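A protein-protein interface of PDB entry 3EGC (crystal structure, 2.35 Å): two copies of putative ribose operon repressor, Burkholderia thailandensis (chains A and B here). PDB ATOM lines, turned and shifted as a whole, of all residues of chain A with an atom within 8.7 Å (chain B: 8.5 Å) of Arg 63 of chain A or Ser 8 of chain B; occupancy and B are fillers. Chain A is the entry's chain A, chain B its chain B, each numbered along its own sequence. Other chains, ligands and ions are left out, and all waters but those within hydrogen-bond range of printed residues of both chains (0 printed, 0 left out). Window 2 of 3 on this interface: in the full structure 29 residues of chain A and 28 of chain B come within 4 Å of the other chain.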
ATOM      1  N   SER A   8      19.372 -22.674  15.617  1.00  0.00           N
ATOM      2  CA  SER A   8      19.570 -23.672  14.539  1.00  0.00           C
ATOM      3  C   SER A   8      20.961 -23.624  13.854  1.00  0.00           C
ATOM      4  O   SER A   8      21.413 -24.596  13.288  1.00  0.00           O
ATOM      5  CB  SER A   8      18.455 -23.570  13.496  1.00  0.00           C
ATOM      6  OG  SER A   8      18.731 -22.559  12.572  1.00  0.00           O
ATOM      7  N   ASN A   9      21.646 -22.495  13.924  1.00  0.00           N
ATOM      8  CA  ASN A   9      22.937 -22.344  13.217  1.00  0.00           C
ATOM      9  C   ASN A   9      22.865 -22.417  11.689  1.00  0.00           C
ATOM     10  O   ASN A   9      23.831 -22.850  11.034  1.00  0.00           O
ATOM     11  CB  ASN A   9      23.985 -23.324  13.721  1.00  0.00           C
ATOM     12  CG  ASN A   9      24.605 -22.893  15.025  1.00  0.00           C
ATOM     13  OD1 ASN A   9      24.332 -23.479  16.054  1.00  0.00           O
ATOM     14  ND2 ASN A   9      25.451 -21.844  14.985  1.00  0.00           N
ATOM     15  N   VAL A  10      21.743 -21.939  11.149  1.00  0.00           N
ATOM     16  CA  VAL A  10      21.519 -21.890   9.719  1.00  0.00           C
ATOM     17  C   VAL A  10      21.091 -20.476   9.424  1.00  0.00           C
ATOM     18  O   VAL A  10      20.242 -19.904  10.069  1.00  0.00           O
ATOM     19  CB  VAL A  10      20.389 -22.832   9.239  1.00  0.00           C
ATOM     20  CG1 VAL A  10      20.211 -22.690   7.671  1.00  0.00           C
ATOM     21  CG2 VAL A  10      20.660 -24.296   9.659  1.00  0.00           C
ATOM     22  N   VAL A  11      21.675 -19.894   8.404  1.00  0.00           N
ATOM     23  CA  VAL A  11      21.282 -18.556   8.046  1.00  0.00           C
ATOM     24  C   VAL A  11      20.864 -18.618   6.584  1.00  0.00           C
ATOM     25  O   VAL A  11      21.388 -19.416   5.854  1.00  0.00           O
ATOM     26  CB  VAL A  11      22.492 -17.646   8.288  1.00  0.00           C
ATOM     27  CG1 VAL A  11      22.551 -16.511   7.323  1.00  0.00           C
ATOM     28  CG2 VAL A  11      22.527 -17.214   9.705  1.00  0.00           C
ATOM     29  N   GLY A  12      19.961 -17.754   6.169  1.00  0.00           N
ATOM     30  CA  GLY A  12      19.450 -17.756   4.800  1.00  0.00           C
ATOM     31  C   GLY A  12      20.175 -16.680   4.005  1.00  0.00           C
ATOM     32  O   GLY A  12      20.268 -15.562   4.494  1.00  0.00           O
ATOM     33  N   LEU A  42      22.081 -21.526   3.705  1.00  0.00           N
ATOM     34  CA  LEU A  42      21.133 -21.946   2.689  1.00  0.00           C
ATOM     35  C   LEU A  42      21.100 -20.863   1.578  1.00  0.00           C
ATOM     36  O   LEU A  42      21.047 -19.637   1.864  1.00  0.00           O
ATOM     37  CB  LEU A  42      19.741 -22.068   3.313  1.00  0.00           C
ATOM     38  CG  LEU A  42      19.207 -23.317   4.004  1.00  0.00           C
ATOM     39  CD1 LEU A  42      17.680 -23.077   4.516  1.00  0.00           C
ATOM     40  CD2 LEU A  42      19.388 -24.572   3.149  1.00  0.00           C
ATOM     41  N   ALA A  56      11.389 -17.090  -1.416  1.00  0.00           N
ATOM     42  CA  ALA A  56      12.558 -17.566  -0.704  1.00  0.00           C
ATOM     43  C   ALA A  56      12.465 -17.183   0.782  1.00  0.00           C
ATOM     44  O   ALA A  56      12.729 -18.027   1.661  1.00  0.00           O
ATOM     45  CB  ALA A  56      13.801 -17.082  -1.326  1.00  0.00           C
ATOM     46  N   VAL A  57      12.057 -15.935   1.055  1.00  0.00           N
ATOM     47  CA  VAL A  57      12.068 -15.423   2.422  1.00  0.00           C
ATOM     48  C   VAL A  57      11.146 -16.330   3.270  1.00  0.00           C
ATOM     49  O   VAL A  57      11.540 -16.813   4.309  1.00  0.00           O
ATOM     50  CB  VAL A  57      11.598 -13.933   2.530  1.00  0.00           C
ATOM     51  CG1 VAL A  57      11.269 -13.560   4.021  1.00  0.00           C
ATOM     52  CG2 VAL A  57      12.662 -12.954   1.992  1.00  0.00           C
ATOM     53  N   GLY A  58       9.932 -16.567   2.773  1.00  0.00           N
ATOM     54  CA  GLY A  58       8.947 -17.441   3.420  1.00  0.00           C
ATOM     55  C   GLY A  58       9.436 -18.878   3.546  1.00  0.00           C
ATOM     56  O   GLY A  58       9.307 -19.499   4.579  1.00  0.00           O
ATOM     57  N   GLN A  59      10.073 -19.374   2.506  1.00  0.00           N
ATOM     58  CA  GLN A  59      10.652 -20.693   2.529  1.00  0.00           C
ATOM     59  C   GLN A  59      11.717 -20.817   3.620  1.00  0.00           C
ATOM     60  O   GLN A  59      11.707 -21.792   4.409  1.00  0.00           O
ATOM     61  CB  GLN A  59      11.216 -20.980   1.161  1.00  0.00           C
ATOM     62  CG  GLN A  59      11.932 -22.276   1.028  1.00  0.00           C
ATOM     63  CD  GLN A  59      12.521 -22.407  -0.330  1.00  0.00           C
ATOM     64  OE1 GLN A  59      11.800 -22.308  -1.333  1.00  0.00           O
ATOM     65  NE2 GLN A  59      13.853 -22.601  -0.394  1.00  0.00           N
ATOM     66  N   PHE A  60      12.591 -19.808   3.694  1.00  0.00           N
ATOM     67  CA  PHE A  60      13.684 -19.792   4.662  1.00  0.00           C
ATOM     68  C   PHE A  60      13.171 -19.589   6.124  1.00  0.00           C
ATOM     69  O   PHE A  60      13.647 -20.201   7.151  1.00  0.00           O
ATOM     70  CB  PHE A  60      14.778 -18.722   4.228  1.00  0.00           C
ATOM     71  CG  PHE A  60      15.680 -19.191   3.063  1.00  0.00           C
ATOM     72  CD1 PHE A  60      15.563 -20.490   2.531  1.00  0.00           C
ATOM     73  CD2 PHE A  60      16.630 -18.372   2.537  1.00  0.00           C
ATOM     74  CE1 PHE A  60      16.372 -20.917   1.500  1.00  0.00           C
ATOM     75  CE2 PHE A  60      17.501 -18.807   1.504  1.00  0.00           C
ATOM     76  CZ  PHE A  60      17.361 -20.068   0.981  1.00  0.00           C
ATOM     77  N   PHE A  61      12.197 -18.719   6.236  1.00  0.00           N
ATOM     78  CA  PHE A  61      11.553 -18.561   7.523  1.00  0.00           C
ATOM     79  C   PHE A  61      10.881 -19.836   8.060  1.00  0.00           C
ATOM     80  O   PHE A  61      11.105 -20.245   9.225  1.00  0.00           O
ATOM     81  CB  PHE A  61      10.595 -17.397   7.504  1.00  0.00           C
ATOM     82  CG  PHE A  61      10.041 -17.090   8.842  1.00  0.00           C
ATOM     83  CD1 PHE A  61      10.891 -16.663   9.860  1.00  0.00           C
ATOM     84  CD2 PHE A  61       8.660 -17.245   9.089  1.00  0.00           C
ATOM     85  CE1 PHE A  61      10.404 -16.383  11.112  1.00  0.00           C
ATOM     86  CE2 PHE A  61       8.152 -16.964  10.364  1.00  0.00           C
ATOM     87  CZ  PHE A  61       9.033 -16.536  11.388  1.00  0.00           C
ATOM     88  N   GLU A  62      10.092 -20.516   7.235  1.00  0.00           N
ATOM     89  CA  GLU A  62       9.471 -21.731   7.708  1.00  0.00           C
ATOM     90  C   GLU A  62      10.496 -22.799   8.089  1.00  0.00           C
ATOM     91  O   GLU A  62      10.276 -23.584   9.004  1.00  0.00           O
ATOM     92  CB  GLU A  62       8.432 -22.285   6.723  1.00  0.00           C
ATOM     93  CG  GLU A  62       8.741 -22.096   5.299  1.00  0.00           C
ATOM     94  CD  GLU A  62       8.774 -23.420   4.531  1.00  0.00           C
ATOM     95  OE1 GLU A  62       7.687 -23.892   4.065  1.00  0.00           O
ATOM     96  OE2 GLU A  62       9.894 -23.980   4.371  1.00  0.00           O
ATOM     97  N   ARG A  63      11.635 -22.826   7.410  1.00  0.00           N
ATOM     98  CA  ARG A  63      12.711 -23.727   7.796  1.00  0.00           C
ATOM     99  C   ARG A  63      13.395 -23.276   9.086  1.00  0.00           C
ATOM    100  O   ARG A  63      14.289 -23.924   9.578  1.00  0.00           O
ATOM    101  CB  ARG A  63      13.755 -23.847   6.663  1.00  0.00           C
ATOM    102  CG  ARG A  63      13.223 -24.619   5.435  1.00  0.00           C
ATOM    103  CD  ARG A  63      14.395 -25.092   4.619  1.00  0.00           C
ATOM    104  NE  ARG A  63      14.034 -26.222   3.774  1.00  0.00           N
ATOM    105  CZ  ARG A  63      14.046 -27.490   4.189  1.00  0.00           C
ATOM    106  NH1 ARG A  63      14.415 -27.762   5.431  1.00  0.00           N
ATOM    107  NH2 ARG A  63      13.698 -28.461   3.356  1.00  0.00           N
ATOM    108  N   ARG A  64      12.940 -22.161   9.625  1.00  0.00           N
ATOM    109  CA  ARG A  64      13.546 -21.532  10.789  1.00  0.00           C
ATOM    110  C   ARG A  64      15.058 -21.364  10.722  1.00  0.00           C
ATOM    111  O   ARG A  64      15.790 -21.894  11.563  1.00  0.00           O
ATOM    112  CB  ARG A  64      13.107 -22.205  12.110  1.00  0.00           C
ATOM    113  CG  ARG A  64      11.583 -22.041  12.466  1.00  0.00           C
ATOM    114  CD  ARG A  64      11.180 -20.579  12.478  1.00  0.00           C
ATOM    115  NE  ARG A  64       9.801 -20.371  12.891  1.00  0.00           N
ATOM    116  CZ  ARG A  64       8.741 -20.630  12.124  1.00  0.00           C
ATOM    117  NH1 ARG A  64       8.924 -21.119  10.916  1.00  0.00           N
ATOM    118  NH2 ARG A  64       7.502 -20.415  12.566  1.00  0.00           N
ATOM    119  N   VAL A  65      15.510 -20.634   9.719  1.00  0.00           N
ATOM    120  CA  VAL A  65      16.863 -20.103   9.731  1.00  0.00           C
ATOM    121  C   VAL A  65      16.944 -19.050  10.838  1.00  0.00           C
ATOM    122  O   VAL A  65      15.933 -18.432  11.196  1.00  0.00           O
ATOM    123  CB  VAL A  65      17.229 -19.443   8.381  1.00  0.00           C
ATOM    124  CG1 VAL A  65      17.265 -20.468   7.262  1.00  0.00           C
ATOM    125  CG2 VAL A  65      16.262 -18.309   8.089  1.00  0.00           C
ATOM    126  N   ASP A  66      18.139 -18.822  11.357  1.00  0.00           N
ATOM    127  CA  ASP A  66      18.295 -17.902  12.477  1.00  0.00           C
ATOM    128  C   ASP A  66      18.136 -16.445  12.036  1.00  0.00           C
ATOM    129  O   ASP A  66      17.863 -15.560  12.827  1.00  0.00           O
ATOM    130  CB  ASP A  66      19.644 -18.135  13.127  1.00  0.00           C
ATOM    131  CG  ASP A  66      19.719 -19.473  13.871  1.00  0.00           C
ATOM    132  OD1 ASP A  66      20.807 -20.019  14.070  1.00  0.00           O
ATOM    133  OD2 ASP A  66      18.688 -19.936  14.317  1.00  0.00           O
ATOM    134  N   PHE A  88      12.954 -11.397  14.051  1.00  0.00           N
ATOM    135  CA  PHE A  88      13.712 -12.065  13.012  1.00  0.00           C
ATOM    136  C   PHE A  88      14.739 -11.104  12.373  1.00  0.00           C
ATOM    137  O   PHE A  88      14.349 -10.168  11.714  1.00  0.00           O
ATOM    138  CB  PHE A  88      12.788 -12.660  11.985  1.00  0.00           C
ATOM    139  CG  PHE A  88      13.481 -13.572  10.997  1.00  0.00           C
ATOM    140  CD1 PHE A  88      13.652 -13.176   9.681  1.00  0.00           C
ATOM    141  CD2 PHE A  88      13.960 -14.803  11.391  1.00  0.00           C
ATOM    142  CE1 PHE A  88      14.254 -13.972   8.794  1.00  0.00           C
ATOM    143  CE2 PHE A  88      14.599 -15.638  10.485  1.00  0.00           C
ATOM    144  CZ  PHE A  88      14.753 -15.216   9.180  1.00  0.00           C
ATOM    145  N   ARG B   7      14.317 -37.255   2.096  1.00  0.00           N
ATOM    146  CA  ARG B   7      13.367 -37.021   3.235  1.00  0.00           C
ATOM    147  C   ARG B   7      13.591 -35.692   3.975  1.00  0.00           C
ATOM    148  O   ARG B   7      12.658 -35.145   4.512  1.00  0.00           O
ATOM    149  CB  ARG B   7      13.314 -38.204   4.207  1.00  0.00           C
ATOM    150  CG  ARG B   7      14.472 -38.269   5.209  1.00  0.00           C
ATOM    151  CD  ARG B   7      14.004 -38.850   6.536  1.00  0.00           C
ATOM    152  NE  ARG B   7      14.798 -39.998   6.965  1.00  0.00           N
ATOM    153  CZ  ARG B   7      14.657 -41.224   6.459  1.00  0.00           C
ATOM    154  NH1 ARG B   7      15.413 -42.225   6.887  1.00  0.00           N
ATOM    155  NH2 ARG B   7      13.758 -41.448   5.503  1.00  0.00           N
ATOM    156  N   SER B   8      14.808 -35.159   3.995  1.00  0.00           N
ATOM    157  CA  SER B   8      14.965 -33.817   4.587  1.00  0.00           C
ATOM    158  C   SER B   8      14.703 -32.662   3.594  1.00  0.00           C
ATOM    159  O   SER B   8      14.466 -31.534   4.007  1.00  0.00           O
ATOM    160  CB  SER B   8      16.338 -33.657   5.259  1.00  0.00           C
ATOM    161  OG  SER B   8      17.343 -33.464   4.295  1.00  0.00           O
ATOM    162  N   ASN B   9      14.757 -32.952   2.295  1.00  0.00           N
ATOM    163  CA  ASN B   9      14.673 -31.938   1.252  1.00  0.00           C
ATOM    164  C   ASN B   9      15.733 -30.823   1.310  1.00  0.00           C
ATOM    165  O   ASN B   9      15.497 -29.664   0.921  1.00  0.00           O
ATOM    166  CB  ASN B   9      13.266 -31.354   1.137  1.00  0.00           C
ATOM    167  CG  ASN B   9      12.272 -32.308   0.404  1.00  0.00           C
ATOM    168  OD1 ASN B   9      11.493 -32.986   1.039  1.00  0.00           O
ATOM    169  ND2 ASN B   9      12.302 -32.329  -0.949  1.00  0.00           N
ATOM    170  N   VAL B  10      16.923 -31.205   1.724  1.00  0.00           N
ATOM    171  CA  VAL B  10      18.041 -30.303   1.671  1.00  0.00           C
ATOM    172  C   VAL B  10      19.171 -31.019   0.982  1.00  0.00           C
ATOM    173  O   VAL B  10      19.482 -32.151   1.294  1.00  0.00           O
ATOM    174  CB  VAL B  10      18.561 -29.895   3.110  1.00  0.00           C
ATOM    175  CG1 VAL B  10      19.726 -28.921   2.989  1.00  0.00           C
ATOM    176  CG2 VAL B  10      17.444 -29.362   3.984  1.00  0.00           C
ATOM    177  N   VAL B  11      19.850 -30.310   0.118  1.00  0.00           N
ATOM    178  CA  VAL B  11      20.960 -30.875  -0.590  1.00  0.00           C
ATOM    179  C   VAL B  11      22.208 -29.986  -0.316  1.00  0.00           C
ATOM    180  O   VAL B  11      22.089 -28.787  -0.124  1.00  0.00           O
ATOM    181  CB  VAL B  11      20.560 -31.008  -2.110  1.00  0.00           C
ATOM    182  CG1 VAL B  11      21.689 -30.707  -3.022  1.00  0.00           C
ATOM    183  CG2 VAL B  11      19.996 -32.440  -2.372  1.00  0.00           C
ATOM    184  N   GLY B  12      23.384 -30.570  -0.283  1.00  0.00           N
ATOM    185  CA  GLY B  12      24.598 -29.814  -0.033  1.00  0.00           C
ATOM    186  C   GLY B  12      25.303 -29.525  -1.361  1.00  0.00           C
ATOM    187  O   GLY B  12      25.490 -30.414  -2.175  1.00  0.00           O
ATOM    188  N   GLY B  38      11.342 -28.425  -4.915  1.00  0.00           N
ATOM    189  CA  GLY B  38      11.060 -28.269  -3.492  1.00  0.00           C
ATOM    190  C   GLY B  38      12.225 -28.637  -2.553  1.00  0.00           C
ATOM    191  O   GLY B  38      12.010 -28.880  -1.343  1.00  0.00           O
ATOM    192  N   TYR B  39      13.454 -28.638  -3.074  1.00  0.00           N
ATOM    193  CA  TYR B  39      14.614 -28.820  -2.214  1.00  0.00           C
ATOM    194  C   TYR B  39      15.292 -27.499  -1.875  1.00  0.00           C
ATOM    195  O   TYR B  39      15.265 -26.521  -2.620  1.00  0.00           O
ATOM    196  CB  TYR B  39      15.673 -29.751  -2.831  1.00  0.00           C
ATOM    197  CG  TYR B  39      15.319 -31.218  -2.913  1.00  0.00           C
ATOM    198  CD1 TYR B  39      14.441 -31.678  -3.864  1.00  0.00           C
ATOM    199  CD2 TYR B  39      15.933 -32.145  -2.087  1.00  0.00           C
ATOM    200  CE1 TYR B  39      14.083 -33.045  -3.960  1.00  0.00           C
ATOM    201  CE2 TYR B  39      15.599 -33.546  -2.201  1.00  0.00           C
ATOM    202  CZ  TYR B  39      14.670 -33.952  -3.159  1.00  0.00           C
ATOM    203  OH  TYR B  39      14.328 -35.267  -3.335  1.00  0.00           O
ATOM    204  N   SER B  40      15.920 -27.482  -0.727  1.00  0.00           N
ATOM    205  CA  SER B  40      16.734 -26.372  -0.351  1.00  0.00           C
ATOM    206  C   SER B  40      18.194 -26.688  -0.589  1.00  0.00           C
ATOM    207  O   SER B  40      18.583 -27.838  -0.616  1.00  0.00           O
ATOM    208  CB  SER B  40      16.538 -26.040   1.136  1.00  0.00           C
ATOM    209  OG  SER B  40      15.288 -25.447   1.326  1.00  0.00           O
ATOM    210  N   VAL B  41      18.991 -25.647  -0.702  1.00  0.00           N
ATOM    211  CA  VAL B  41      20.411 -25.786  -1.019  1.00  0.00           C
ATOM    212  C   VAL B  41      21.318 -25.099   0.007  1.00  0.00           C
ATOM    213  O   VAL B  41      21.274 -23.873   0.171  1.00  0.00           O
ATOM    214  CB  VAL B  41      20.739 -25.264  -2.442  1.00  0.00           C
ATOM    215  CG1 VAL B  41      22.242 -25.416  -2.754  1.00  0.00           C
ATOM    216  CG2 VAL B  41      19.864 -25.971  -3.466  1.00  0.00           C
ATOM    217  N   LEU B  42      22.097 -25.925   0.693  1.00  0.00           N
ATOM    218  CA  LEU B  42      23.152 -25.490   1.597  1.00  0.00           C
ATOM    219  C   LEU B  42      24.439 -25.244   0.794  1.00  0.00           C
ATOM    220  O   LEU B  42      24.878 -26.098   0.066  1.00  0.00           O
ATOM    221  CB  LEU B  42      23.415 -26.550   2.678  1.00  0.00           C
ATOM    222  CG  LEU B  42      22.663 -26.623   3.999  1.00  0.00           C
ATOM    223  CD1 LEU B  42      23.265 -27.742   4.918  1.00  0.00           C
ATOM    224  CD2 LEU B  42      22.570 -25.282   4.818  1.00  0.00           C
ATOM    225  N   PHE B  60      28.086 -31.108   6.147  1.00  0.00           N
ATOM    226  CA  PHE B  60      26.826 -31.263   5.430  1.00  0.00           C
ATOM    227  C   PHE B  60      26.230 -32.640   5.755  1.00  0.00           C
ATOM    228  O   PHE B  60      24.995 -32.742   5.977  1.00  0.00           O
ATOM    229  CB  PHE B  60      27.002 -31.016   3.914  1.00  0.00           C
ATOM    230  CG  PHE B  60      27.091 -29.577   3.533  1.00  0.00           C
ATOM    231  CD1 PHE B  60      26.954 -28.570   4.488  1.00  0.00           C
ATOM    232  CD2 PHE B  60      27.278 -29.210   2.187  1.00  0.00           C
ATOM    233  CE1 PHE B  60      27.044 -27.236   4.151  1.00  0.00           C
ATOM    234  CE2 PHE B  60      27.360 -27.855   1.819  1.00  0.00           C
ATOM    235  CZ  PHE B  60      27.244 -26.852   2.802  1.00  0.00           C
ATOM    236  N   ARG B  63      24.584 -32.789   9.114  1.00  0.00           N
ATOM    237  CA  ARG B  63      23.362 -32.027   9.078  1.00  0.00           C
ATOM    238  C   ARG B  63      22.312 -32.840   8.351  1.00  0.00           C
ATOM    239  O   ARG B  63      21.172 -32.390   8.154  1.00  0.00           O
ATOM    240  CB  ARG B  63      23.579 -30.706   8.348  1.00  0.00           C
ATOM    241  CG  ARG B  63      24.271 -29.650   9.164  1.00  0.00           C
ATOM    242  CD  ARG B  63      23.870 -28.252   8.663  1.00  0.00           C
ATOM    243  NE  ARG B  63      24.103 -27.245   9.682  1.00  0.00           N
ATOM    244  CZ  ARG B  63      23.200 -26.862  10.582  1.00  0.00           C
ATOM    245  NH1 ARG B  63      21.987 -27.384  10.548  1.00  0.00           N
ATOM    246  NH2 ARG B  63      23.501 -25.910  11.469  1.00  0.00           N
ATOM    247  N   ARG B  64      22.720 -34.028   7.921  1.00  0.00           N
ATOM    248  CA  ARG B  64      21.883 -34.915   7.112  1.00  0.00           C
ATOM    249  C   ARG B  64      21.159 -34.331   5.930  1.00  0.00           C
ATOM    250  O   ARG B  64      19.964 -34.519   5.798  1.00  0.00           O
ATOM    251  CB  ARG B  64      20.904 -35.718   7.993  1.00  0.00           C
ATOM    252  CG  ARG B  64      21.666 -36.685   8.932  1.00  0.00           C
ATOM    253  CD  ARG B  64      22.683 -37.554   8.180  1.00  0.00           C
ATOM    254  NE  ARG B  64      23.182 -38.677   8.976  1.00  0.00           N
ATOM    255  CZ  ARG B  64      24.146 -38.596   9.899  1.00  0.00           C
ATOM    256  NH1 ARG B  64      24.721 -37.422  10.184  1.00  0.00           N
ATOM    257  NH2 ARG B  64      24.522 -39.703  10.575  1.00  0.00           N
ATOM    258  N   VAL B  65      21.893 -33.632   5.080  1.00  0.00           N
ATOM    259  CA  VAL B  65      21.433 -33.368   3.732  1.00  0.00           C
ATOM    260  C   VAL B  65      21.121 -34.683   3.048  1.00  0.00           C
ATOM    261  O   VAL B  65      21.744 -35.696   3.350  1.00  0.00           O
ATOM    262  CB  VAL B  65      22.515 -32.615   2.906  1.00  0.00           C
ATOM    263  CG1 VAL B  65      22.753 -31.228   3.537  1.00  0.00           C
ATOM    264  CG2 VAL B  65      23.835 -33.424   2.870  1.00  0.00           C
ATOM    265  N   ASP B  66      20.163 -34.667   2.135  1.00  0.00           N
ATOM    266  CA  ASP B  66      19.822 -35.852   1.357  1.00  0.00           C
ATOM    267  C   ASP B  66      20.899 -36.322   0.385  1.00  0.00           C
ATOM    268  O   ASP B  66      20.895 -37.477  -0.038  1.00  0.00           O
ATOM    269  CB  ASP B  66      18.526 -35.622   0.600  1.00  0.00           C
ATOM    270  CG  ASP B  66      17.342 -35.464   1.521  1.00  0.00           C
ATOM    271  OD1 ASP B  66      16.374 -34.781   1.136  1.00  0.00           O
ATOM    272  OD2 ASP B  66      17.404 -36.041   2.643  1.00  0.00           O
ATOM    273  N   GLY B  67      21.820 -35.426   0.036  1.00  0.00           N
ATOM    274  CA  GLY B  67      22.791 -35.695  -1.026  1.00  0.00           C
ATOM    275  C   GLY B  67      23.658 -34.476  -1.285  1.00  0.00           C
ATOM    276  O   GLY B  67      23.369 -33.397  -0.770  1.00  0.00           O
ATOM    277  N   PHE B  88      24.822 -42.814   0.624  1.00  0.00           N
ATOM    278  CA  PHE B  88      24.812 -41.364   0.544  1.00  0.00           C
ATOM    279  C   PHE B  88      25.186 -40.896  -0.884  1.00  0.00           C
ATOM    280  O   PHE B  88      26.306 -41.023  -1.289  1.00  0.00           O
ATOM    281  CB  PHE B  88      25.755 -40.751   1.584  1.00  0.00           C
ATOM    282  CG  PHE B  88      25.652 -39.265   1.674  1.00  0.00           C
ATOM    283  CD1 PHE B  88      26.682 -38.453   1.254  1.00  0.00           C
ATOM    284  CD2 PHE B  88      24.505 -38.668   2.188  1.00  0.00           C
ATOM    285  CE1 PHE B  88      26.590 -37.106   1.374  1.00  0.00           C
ATOM    286  CE2 PHE B  88      24.409 -37.298   2.268  1.00  0.00           C
ATOM    287  CZ  PHE B  88      25.441 -36.527   1.882  1.00  0.00           C
ATOM    288  N   ILE B 256      18.296 -39.813  -4.847  1.00  0.00           N
ATOM    289  CA  ILE B 256      17.721 -39.657  -3.475  1.00  0.00           C
ATOM    290  C   ILE B 256      16.349 -40.332  -3.342  1.00  0.00           C
ATOM    291  O   ILE B 256      16.036 -40.944  -2.312  1.00  0.00           O
ATOM    292  CB  ILE B 256      17.537 -38.164  -3.101  1.00  0.00           C
ATOM    293  CG1 ILE B 256      18.913 -37.463  -2.967  1.00  0.00           C
ATOM    294  CG2 ILE B 256      16.682 -38.022  -1.832  1.00  0.00           C
ATOM    295  CD1 ILE B 256      18.848 -35.965  -3.063  1.00  0.00           C
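Of the 19 printed residues of chain B, 7 touch a printed residue of chain A. Printed residues of chain A that touch a printed residue of chain B: Ser 8, Asn 9, Val 10, Leu 42, Gln 59 and Arg 63. Hydrophobic or aromatic side chains of chain A within 4 Å of the printed part of chain B: Val 10 and Leu 42. Among the printed residues, 11 pairs touch across the chains.
O of Ser 8 of chain A sits at hydrogen-bond distance from NH2 of Arg 63 of chain B (3.1 Å). The guanidinium group (NH2) of Arg 63 of chain B lies within hydrogen-bond range of the backbone carbonyl oxygen (O) of Asn 9 of chain A (3.1 Å). The guanidinium group (NH2) of Arg 63 of chain A lies within hydrogen-bond range of the backbone carbonyl oxygen (O) of Ser 8 of chain B (3.2 Å). The guanidinium group (NH2) of Arg 63 of chain A is in hydrogen-bond range of the backbone carbonyl oxygen (O) of Asn 9 of chain B, at 3.3 Å. The guanidinium group (NE) of Arg 63 of chain A is in hydrogen-bond range of the side-chain hydroxyl (OG) of Ser 40 of chain B, at 2.9 Å.
Of chain B, only Ser 8 (3.2 Å), Asn 9 (3.3 Å), Val 10 (3.7 Å) and Ser 40 (2.9 Å) come within 4 Å of Arg 63 of chain A. Of chain A, only Arg 63 (3.2 Å) comes within 4 Å of Ser 8 of chain B. Printed residues of chain B within 4 Å of Gln 59 of chain A: Ser 40 (3.6 Å). Of the printed residues of chain B, Ser 8 of chain A touches Arg 63. Of the printed residues of chain A, Val 10 of chain B touches Arg 63. Of the printed residues of chain A, Arg 63 of chain B touches Ser 8, Asn 9 and Val 10. Val 11 of chain B touches none of the printed residues of chain A. Val 11 of chain A touches none of the printed residues of chain B. The nearest residue of chain A that does not touch Ser 8 of chain B is Leu 42 of chain A (8.6 Å). The nearest printed residue of chain A that does not touch Asn 9 of chain B is Leu 42 of chain A (6.8 Å).
Ser 8 of chain A touches Arg 63 of chain B, and with the chains exchanged Arg 63 of chain A touches Ser 8 of chain B. Asn 9 of chain A touches Arg 63 of chain B, and with the chains exchanged Arg 63 of chain A touches Asn 9 of chain B. Val 10 of chain A touches Arg 63 of chain B, and with the chains exchanged Arg 63 of chain A touches Val 10 of chain B. Leu 42 of chain B touches its own counterpart, Leu 42 of chain A. Positions printed for both chains: 8, 9, 10, 11, 12, 42, 60, 63, 64, 65, 66 and 88. Of the 11 pairs that touch across the chains among the printed residues, 7 have their exchanged pair printed and touching as well.
OD1 of Asp 66 of chain A is in hydrogen-bond range of N of Asn 9 of chain A (2.6 Å). OD2 of Asp 66 of chain B sits at hydrogen-bond distance from N of Ser 8 of chain B. N of Ser 40 of chain B lies within hydrogen-bond range of O of Asn 9 of chain B (2.8 Å). The backbone carbonyl oxygen (O) of Val 10 of chain B is in hydrogen-bond range of the backbone NH (N) of Asp 66 of chain B. The backbone carbonyl oxygen (O) of Ser 40 of chain B is in hydrogen-bond range of the backbone NH (N) of Val 11 of chain B (2.9 Å). The backbone carbonyl oxygen of Val 11 of chain B lies within hydrogen-bond range of the backbone NH of Leu 42 of chain B, at 3.0 Å.
CG2 of Val 10 of chain A touches NH1 of Arg 63 of chain B (3.5 Å). CD2 of Leu 42 of chain A touches CB of Ser 40 of chain B (3.8 Å). Leu 42 of chain A touches Val 41 of chain B. Leu 42 of chain B touches Leu 42 of chain A. Gln 59 of chain A touches Ser 40 of chain B (NE2 to OG, 3.6 Å). Val 10 of chain B touches Arg 63 of chain A (CG2 to NH1, 3.7 Å).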
